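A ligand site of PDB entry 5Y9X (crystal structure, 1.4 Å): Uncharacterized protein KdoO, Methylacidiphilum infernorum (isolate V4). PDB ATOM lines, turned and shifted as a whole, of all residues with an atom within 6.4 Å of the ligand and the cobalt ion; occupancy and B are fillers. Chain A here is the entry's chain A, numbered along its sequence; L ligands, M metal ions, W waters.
The guanidinium group (NH1) of Arg 162 is in salt-bridge range of an oxygen (O1) of the ligand, at 3.2 Å.
NE of Arg 174 is in salt-bridge range of O5 of the ligand, 2.7 Å away.
The indole nitrogen of Trp 176 sits at hydrogen-bond distance from an oxygen (O5) of the ligand (2.8 Å).
O1 of the ligand lies within salt-bridge range of NH1 of Arg 127, 2.8 Å away.
The cobalt ion is bound by OD1 of Asp 148 (2.1 Å), O2 of the ligand (2.1 Å), NE2 of His 260 (2.1 Å), NE2 of His 146 (2.2 Å), water W3 (2.2 Å) and O3 of the ligand (2.2 Å).
The side-chain carboxylate (OD2) of Asp 142 lies close to an oxygen (O3) of the ligand, 3.2 Å away.
Phe 164 touches the ligand (CE2 to O1, 3.5 Å).
CG2 of Val 262 touches O5 of the ligand, at 3.6 Å.
CD2 of Leu 268 touches O4 of the ligand (3.7 Å).
Hydrophobic or aromatic side chains that line the ligand: His 146, Phe 164, Trp 176, His 260, Val 262 and Leu 268.
11 residues have an atom within 4 Å of the ligand: Arg 127, Asp 142, His 146, Asp 148, Arg 162, Phe 164, Arg 174, Trp 176, His 260, Val 262 and Leu 268.
Within 4 Å of the cobalt ion: His 146, Asp 148 and His 260.
OE1 of Glu 270 lies within salt-bridge range of NH2 of Arg 127 (3.4 Å).
The side-chain carboxylate of Asp 148 lies within salt-bridge range of the guanidinium group of Arg 162 (3.2 Å).
The side-chain carboxylate of Asp 148 sits at hydrogen-bond distance from the side-chain hydroxyl of Thr 255 (2.7 Å).
The backbone carbonyl oxygen of Leu 268 is in hydrogen-bond range of the backbone NH of Arg 127 (2.9 Å).
The backbone NH of Phe 164 lies within hydrogen-bond range of the backbone carbonyl oxygen of Trp 251 (2.8 Å).
O of Asp 142 sits at hydrogen-bond distance from N of Val 262.
OE2 of Glu 270 lies within salt-bridge range of NE of Arg 162 (3.1 Å).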
ATOM      1  N   ARG A 127     -13.586  -0.955 -14.425  1.00  0.00           N
ATOM      2  CA  ARG A 127     -14.557   0.034 -13.964  1.00  0.00           C
ATOM      3  C   ARG A 127     -14.324   0.309 -12.489  1.00  0.00           C
ATOM      4  O   ARG A 127     -14.873  -0.372 -11.612  1.00  0.00           O
ATOM      5  CB  ARG A 127     -15.990  -0.432 -14.242  1.00  0.00           C
ATOM      6  CG  ARG A 127     -16.167  -0.933 -15.653  1.00  0.00           C
ATOM      7  CD  ARG A 127     -17.597  -1.347 -15.933  1.00  0.00           C
ATOM      8  NE  ARG A 127     -17.778  -1.795 -17.310  1.00  0.00           N
ATOM      9  CZ  ARG A 127     -18.870  -2.420 -17.738  1.00  0.00           C
ATOM     10  NH1 ARG A 127     -19.876  -2.668 -16.906  1.00  0.00           N
ATOM     11  NH2 ARG A 127     -18.961  -2.795 -19.006  1.00  0.00           N
ATOM     12  N   ILE A 131     -20.754   2.907  -8.590  1.00  0.00           N
ATOM     13  CA  ILE A 131     -21.964   3.036  -9.405  1.00  0.00           C
ATOM     14  C   ILE A 131     -22.973   3.994  -8.755  1.00  0.00           C
ATOM     15  O   ILE A 131     -23.650   4.754  -9.460  1.00  0.00           O
ATOM     16  CB  ILE A 131     -22.592   1.649  -9.635  1.00  0.00           C
ATOM     17  CG1 ILE A 131     -21.735   0.836 -10.600  1.00  0.00           C
ATOM     18  CG2 ILE A 131     -24.035   1.766 -10.149  1.00  0.00           C
ATOM     19  CD1 ILE A 131     -21.737   1.354 -12.009  1.00  0.00           C
ATOM     20  N   ASP A 142     -27.359   3.180 -16.732  1.00  0.00           N
ATOM     21  CA  ASP A 142     -27.454   1.730 -16.622  1.00  0.00           C
ATOM     22  C   ASP A 142     -28.066   1.259 -15.308  1.00  0.00           C
ATOM     23  O   ASP A 142     -28.046   0.054 -15.033  1.00  0.00           O
ATOM     24  CB  ASP A 142     -26.111   1.069 -16.928  1.00  0.00           C
ATOM     25  CG  ASP A 142     -25.833   0.993 -18.423  1.00  0.00           C
ATOM     26  OD1 ASP A 142     -26.752   1.274 -19.227  1.00  0.00           O
ATOM     27  OD2 ASP A 142     -24.699   0.636 -18.798  1.00  0.00           O
ATOM     28  N   HIS A 146     -32.044  -2.728 -19.457  1.00  0.00           N
ATOM     29  CA  HIS A 146     -31.793  -2.616 -20.882  1.00  0.00           C
ATOM     30  C   HIS A 146     -31.131  -3.900 -21.364  1.00  0.00           C
ATOM     31  O   HIS A 146     -30.602  -4.684 -20.576  1.00  0.00           O
ATOM     32  CB  HIS A 146     -30.862  -1.435 -21.162  1.00  0.00           C
ATOM     33  CG  HIS A 146     -29.497  -1.633 -20.573  1.00  0.00           C
ATOM     34  ND1 HIS A 146     -29.232  -1.441 -19.230  1.00  0.00           N
ATOM     35  CD2 HIS A 146     -28.334  -2.052 -21.130  1.00  0.00           C
ATOM     36  CE1 HIS A 146     -27.966  -1.732 -18.983  1.00  0.00           C
ATOM     37  NE2 HIS A 146     -27.392  -2.109 -20.125  1.00  0.00           N
ATOM     38  N   VAL A 147     -31.188  -4.109 -22.682  1.00  0.00           N
ATOM     39  CA  VAL A 147     -30.242  -4.968 -23.373  1.00  0.00           C
ATOM     40  C   VAL A 147     -29.172  -4.079 -23.985  1.00  0.00           C
ATOM     41  O   VAL A 147     -29.410  -2.891 -24.266  1.00  0.00           O
ATOM     42  CB  VAL A 147     -30.905  -5.858 -24.445  1.00  0.00           C
ATOM     43  CG1 VAL A 147     -31.891  -6.801 -23.805  1.00  0.00           C
ATOM     44  CG2 VAL A 147     -31.558  -5.004 -25.532  1.00  0.00           C
ATOM     45  N   ASP A 148     -27.981  -4.626 -24.178  1.00  0.00           N
ATOM     46  CA  ASP A 148     -26.849  -3.827 -24.645  1.00  0.00           C
ATOM     47  C   ASP A 148     -26.976  -3.522 -26.130  1.00  0.00           C
ATOM     48  O   ASP A 148     -27.219  -4.408 -26.954  1.00  0.00           O
ATOM     49  CB  ASP A 148     -25.530  -4.532 -24.371  1.00  0.00           C
ATOM     50  CG  ASP A 148     -25.085  -4.395 -22.929  1.00  0.00           C
ATOM     51  OD1 ASP A 148     -25.745  -3.668 -22.146  1.00  0.00           O
ATOM     52  OD2 ASP A 148     -24.066  -5.022 -22.594  1.00  0.00           O
ATOM     53  N   PHE A 150     -25.105  -0.211 -28.619  1.00  0.00           N
ATOM     54  CA  PHE A 150     -24.236   0.945 -28.509  1.00  0.00           C
ATOM     55  C   PHE A 150     -24.314   1.734 -29.808  1.00  0.00           C
ATOM     56  O   PHE A 150     -23.995   1.189 -30.882  1.00  0.00           O
ATOM     57  CB  PHE A 150     -22.803   0.493 -28.202  1.00  0.00           C
ATOM     58  CG  PHE A 150     -22.721  -0.325 -26.955  1.00  0.00           C
ATOM     59  CD1 PHE A 150     -22.810   0.273 -25.706  1.00  0.00           C
ATOM     60  CD2 PHE A 150     -22.611  -1.711 -27.012  1.00  0.00           C
ATOM     61  CE1 PHE A 150     -22.760  -0.478 -24.543  1.00  0.00           C
ATOM     62  CE2 PHE A 150     -22.561  -2.471 -25.850  1.00  0.00           C
ATOM     63  CZ  PHE A 150     -22.626  -1.849 -24.618  1.00  0.00           C
ATOM     64  N   ARG A 162     -20.798 -11.242 -22.413  1.00  0.00           N
ATOM     65  CA  ARG A 162     -19.936 -10.567 -21.450  1.00  0.00           C
ATOM     66  C   ARG A 162     -19.629 -11.446 -20.259  1.00  0.00           C
ATOM     67  O   ARG A 162     -20.510 -12.155 -19.741  1.00  0.00           O
ATOM     68  CB  ARG A 162     -20.511  -9.216 -21.026  1.00  0.00           C
ATOM     69  CG  ARG A 162     -20.563  -8.223 -22.174  1.00  0.00           C
ATOM     70  CD  ARG A 162     -20.964  -6.813 -21.760  1.00  0.00           C
ATOM     71  NE  ARG A 162     -20.336  -5.840 -22.647  1.00  0.00           N
ATOM     72  CZ  ARG A 162     -20.460  -4.522 -22.564  1.00  0.00           C
ATOM     73  NH1 ARG A 162     -21.242  -3.975 -21.630  1.00  0.00           N
ATOM     74  NH2 ARG A 162     -19.803  -3.740 -23.413  1.00  0.00           N
ATOM     75  N   PHE A 164     -18.027 -11.027 -16.362  1.00  0.00           N
ATOM     76  CA  PHE A 164     -17.889  -9.981 -15.348  1.00  0.00           C
ATOM     77  C   PHE A 164     -17.250 -10.600 -14.120  1.00  0.00           C
ATOM     78  O   PHE A 164     -17.589 -11.720 -13.735  1.00  0.00           O
ATOM     79  CB  PHE A 164     -19.272  -9.495 -14.903  1.00  0.00           C
ATOM     80  CG  PHE A 164     -20.054  -8.768 -15.946  1.00  0.00           C
ATOM     81  CD1 PHE A 164     -20.957  -9.435 -16.767  1.00  0.00           C
ATOM     82  CD2 PHE A 164     -19.920  -7.391 -16.088  1.00  0.00           C
ATOM     83  CE1 PHE A 164     -21.713  -8.739 -17.705  1.00  0.00           C
ATOM     84  CE2 PHE A 164     -20.666  -6.695 -17.031  1.00  0.00           C
ATOM     85  CZ  PHE A 164     -21.565  -7.373 -17.845  1.00  0.00           C
ATOM     86  N   ARG A 174     -21.805  -6.333  -6.041  1.00  0.00           N
ATOM     87  CA  ARG A 174     -22.251  -5.542  -7.176  1.00  0.00           C
ATOM     88  C   ARG A 174     -23.730  -5.827  -7.353  1.00  0.00           C
ATOM     89  O   ARG A 174     -24.119  -6.968  -7.640  1.00  0.00           O
ATOM     90  CB  ARG A 174     -21.461  -5.855  -8.435  1.00  0.00           C
ATOM     91  CG  ARG A 174     -21.638  -4.765  -9.486  1.00  0.00           C
ATOM     92  CD  ARG A 174     -20.489  -4.699 -10.395  1.00  0.00           C
ATOM     93  NE  ARG A 174     -20.499  -3.578 -11.325  1.00  0.00           N
ATOM     94  CZ  ARG A 174     -19.783  -2.456 -11.176  1.00  0.00           C
ATOM     95  NH1 ARG A 174     -19.026  -2.291 -10.101  1.00  0.00           N
ATOM     96  NH2 ARG A 174     -19.815  -1.519 -12.111  1.00  0.00           N
ATOM     97  N   SER A 175     -24.553  -4.807  -7.152  1.00  0.00           N
ATOM     98  CA  SER A 175     -26.004  -4.991  -7.076  1.00  0.00           C
ATOM     99  C   SER A 175     -26.598  -4.846  -8.474  1.00  0.00           C
ATOM    100  O   SER A 175     -26.566  -3.748  -9.049  1.00  0.00           O
ATOM    101  CB  SER A 175     -26.615  -3.983  -6.115  1.00  0.00           C
ATOM    102  OG  SER A 175     -26.150  -4.210  -4.788  1.00  0.00           O
ATOM    103  N   TRP A 176     -27.121  -5.937  -9.014  1.00  0.00           N
ATOM    104  CA  TRP A 176     -27.798  -5.953 -10.296  1.00  0.00           C
ATOM    105  C   TRP A 176     -29.301  -6.133 -10.108  1.00  0.00           C
ATOM    106  O   TRP A 176     -29.780  -6.599  -9.075  1.00  0.00           O
ATOM    107  CB  TRP A 176     -27.288  -7.110 -11.153  1.00  0.00           C
ATOM    108  CG  TRP A 176     -26.137  -6.779 -12.055  1.00  0.00           C
ATOM    109  CD1 TRP A 176     -25.138  -5.880 -11.821  1.00  0.00           C
ATOM    110  CD2 TRP A 176     -25.881  -7.343 -13.338  1.00  0.00           C
ATOM    111  NE1 TRP A 176     -24.256  -5.872 -12.890  1.00  0.00           N
ATOM    112  CE2 TRP A 176     -24.706  -6.749 -13.843  1.00  0.00           C
ATOM    113  CE3 TRP A 176     -26.545  -8.304 -14.123  1.00  0.00           C
ATOM    114  CZ2 TRP A 176     -24.172  -7.073 -15.090  1.00  0.00           C
ATOM    115  CZ3 TRP A 176     -26.020  -8.630 -15.367  1.00  0.00           C
ATOM    116  CH2 TRP A 176     -24.847  -8.012 -15.843  1.00  0.00           C
ATOM    117  N   HIS A 225     -33.411  -0.581 -26.432  1.00  0.00           N
ATOM    118  CA  HIS A 225     -32.582  -0.063 -25.364  1.00  0.00           C
ATOM    119  C   HIS A 225     -33.070   1.314 -24.907  1.00  0.00           C
ATOM    120  O   HIS A 225     -33.364   1.528 -23.721  1.00  0.00           O
ATOM    121  CB  HIS A 225     -31.132   0.014 -25.893  1.00  0.00           C
ATOM    122  CG  HIS A 225     -30.155   0.682 -24.972  1.00  0.00           C
ATOM    123  ND1 HIS A 225     -30.052   2.058 -24.878  1.00  0.00           N
ATOM    124  CD2 HIS A 225     -29.199   0.174 -24.152  1.00  0.00           C
ATOM    125  CE1 HIS A 225     -29.079   2.362 -24.027  1.00  0.00           C
ATOM    126  NE2 HIS A 225     -28.557   1.240 -23.569  1.00  0.00           N
ATOM    127  N   TRP A 251     -19.585 -13.750 -13.361  1.00  0.00           N
ATOM    128  CA  TRP A 251     -20.808 -14.154 -14.032  1.00  0.00           C
ATOM    129  C   TRP A 251     -20.699 -13.930 -15.527  1.00  0.00           C
ATOM    130  O   TRP A 251     -19.885 -13.132 -15.997  1.00  0.00           O
ATOM    131  CB  TRP A 251     -22.057 -13.518 -13.406  1.00  0.00           C
ATOM    132  CG  TRP A 251     -22.141 -12.007 -13.402  1.00  0.00           C
ATOM    133  CD1 TRP A 251     -22.944 -11.233 -14.193  1.00  0.00           C
ATOM    134  CD2 TRP A 251     -21.459 -11.098 -12.513  1.00  0.00           C
ATOM    135  NE1 TRP A 251     -22.786  -9.902 -13.877  1.00  0.00           N
ATOM    136  CE2 TRP A 251     -21.890  -9.792 -12.852  1.00  0.00           C
ATOM    137  CE3 TRP A 251     -20.534 -11.265 -11.478  1.00  0.00           C
ATOM    138  CZ2 TRP A 251     -21.411  -8.656 -12.194  1.00  0.00           C
ATOM    139  CZ3 TRP A 251     -20.068 -10.138 -10.828  1.00  0.00           C
ATOM    140  CH2 TRP A 251     -20.506  -8.849 -11.189  1.00  0.00           C
ATOM    141  N   THR A 255     -25.540 -10.082 -22.843  1.00  0.00           N
ATOM    142  CA  THR A 255     -26.154  -8.832 -22.388  1.00  0.00           C
ATOM    143  C   THR A 255     -27.009  -8.162 -23.466  1.00  0.00           C
ATOM    144  O   THR A 255     -27.729  -7.204 -23.144  1.00  0.00           O
ATOM    145  CB  THR A 255     -25.097  -7.855 -21.886  1.00  0.00           C
ATOM    146  OG1 THR A 255     -24.115  -7.681 -22.900  1.00  0.00           O
ATOM    147  CG2 THR A 255     -24.446  -8.369 -20.620  1.00  0.00           C
ATOM    148  N   HIS A 260     -30.813  -6.151 -17.937  1.00  0.00           N
ATOM    149  CA  HIS A 260     -29.990  -5.985 -16.757  1.00  0.00           C
ATOM    150  C   HIS A 260     -29.874  -4.508 -16.416  1.00  0.00           C
ATOM    151  O   HIS A 260     -30.121  -3.621 -17.253  1.00  0.00           O
ATOM    152  CB  HIS A 260     -28.610  -6.629 -16.943  1.00  0.00           C
ATOM    153  CG  HIS A 260     -27.845  -6.045 -18.091  1.00  0.00           C
ATOM    154  ND1 HIS A 260     -28.141  -6.346 -19.409  1.00  0.00           N
ATOM    155  CD2 HIS A 260     -26.857  -5.128 -18.137  1.00  0.00           C
ATOM    156  CE1 HIS A 260     -27.354  -5.642 -20.209  1.00  0.00           C
ATOM    157  NE2 HIS A 260     -26.557  -4.902 -19.460  1.00  0.00           N
ATOM    158  N   ALA A 261     -29.501  -4.252 -15.163  1.00  0.00           N
ATOM    159  CA  ALA A 261     -29.244  -2.923 -14.635  1.00  0.00           C
ATOM    160  C   ALA A 261     -28.324  -3.086 -13.430  1.00  0.00           C
ATOM    161  O   ALA A 261     -28.307  -4.142 -12.802  1.00  0.00           O
ATOM    162  CB  ALA A 261     -30.538  -2.242 -14.180  1.00  0.00           C
ATOM    163  N   VAL A 262     -27.553  -2.048 -13.122  1.00  0.00           N
ATOM    164  CA  VAL A 262     -26.680  -2.071 -11.958  1.00  0.00           C
ATOM    165  C   VAL A 262     -27.018  -0.883 -11.071  1.00  0.00           C
ATOM    166  O   VAL A 262     -27.188   0.242 -11.574  1.00  0.00           O
ATOM    167  CB  VAL A 262     -25.191  -2.104 -12.349  1.00  0.00           C
ATOM    168  CG1 VAL A 262     -24.812  -0.910 -13.215  1.00  0.00           C
ATOM    169  CG2 VAL A 262     -24.303  -2.197 -11.094  1.00  0.00           C
ATOM    170  N   LEU A 268     -14.833  -3.479 -11.012  1.00  0.00           N
ATOM    171  CA  LEU A 268     -15.339  -4.557 -11.846  1.00  0.00           C
ATOM    172  C   LEU A 268     -14.405  -4.708 -13.026  1.00  0.00           C
ATOM    173  O   LEU A 268     -13.962  -3.714 -13.615  1.00  0.00           O
ATOM    174  CB  LEU A 268     -16.738  -4.178 -12.383  1.00  0.00           C
ATOM    175  CG  LEU A 268     -17.463  -5.196 -13.253  1.00  0.00           C
ATOM    176  CD1 LEU A 268     -18.035  -6.311 -12.408  1.00  0.00           C
ATOM    177  CD2 LEU A 268     -18.559  -4.523 -14.100  1.00  0.00           C
ATOM    178  N   GLU A 270     -14.525  -6.556 -16.821  1.00  0.00           N
ATOM    179  CA  GLU A 270     -15.510  -7.047 -17.759  1.00  0.00           C
ATOM    180  C   GLU A 270     -14.811  -7.360 -19.078  1.00  0.00           C
ATOM    181  O   GLU A 270     -13.904  -6.630 -19.503  1.00  0.00           O
ATOM    182  CB  GLU A 270     -16.646  -6.027 -17.941  1.00  0.00           C
ATOM    183  CG  GLU A 270     -17.720  -6.403 -18.951  1.00  0.00           C
ATOM    184  CD  GLU A 270     -17.361  -5.993 -20.364  1.00  0.00           C
ATOM    185  OE1 GLU A 270     -16.736  -4.925 -20.552  1.00  0.00           O
ATOM    186  OE2 GLU A 270     -17.695  -6.748 -21.289  1.00  0.00           O
HETATM  187  C1  LIG L   1     -23.069  -3.531 -18.793  1.00  0.00           C
HETATM  188  O1  LIG L   1     -21.858  -3.795 -18.539  1.00  0.00           O
HETATM  189  O2  LIG L   1     -23.605  -3.892 -19.872  1.00  0.00           O
HETATM  190  C2  LIG L   1     -23.890  -2.761 -17.808  1.00  0.00           C
HETATM  191  O3  LIG L   1     -25.059  -2.479 -18.088  1.00  0.00           O
HETATM  192  C3  LIG L   1     -23.314  -2.367 -16.495  1.00  0.00           C
HETATM  193  C4  LIG L   1     -23.114  -3.479 -15.526  1.00  0.00           C
HETATM  194  C5  LIG L   1     -22.221  -3.191 -14.376  1.00  0.00           C
HETATM  195  O4  LIG L   1     -21.452  -2.185 -14.395  1.00  0.00           O
HETATM  196  O5  LIG L   1     -22.206  -3.958 -13.378  1.00  0.00           O
HETATM  197 CO    CO M   1     -25.525  -3.175 -20.166  1.00  0.00          CO
HETATM  198  O   HOH W   1     -21.601   0.409 -15.438  1.00  0.00           O
HETATM  199  O   HOH W   2     -22.097   0.432 -18.150  1.00  0.00           O
HETATM  200  O   HOH W   3     -24.598  -1.294 -20.895  1.00  0.00           O
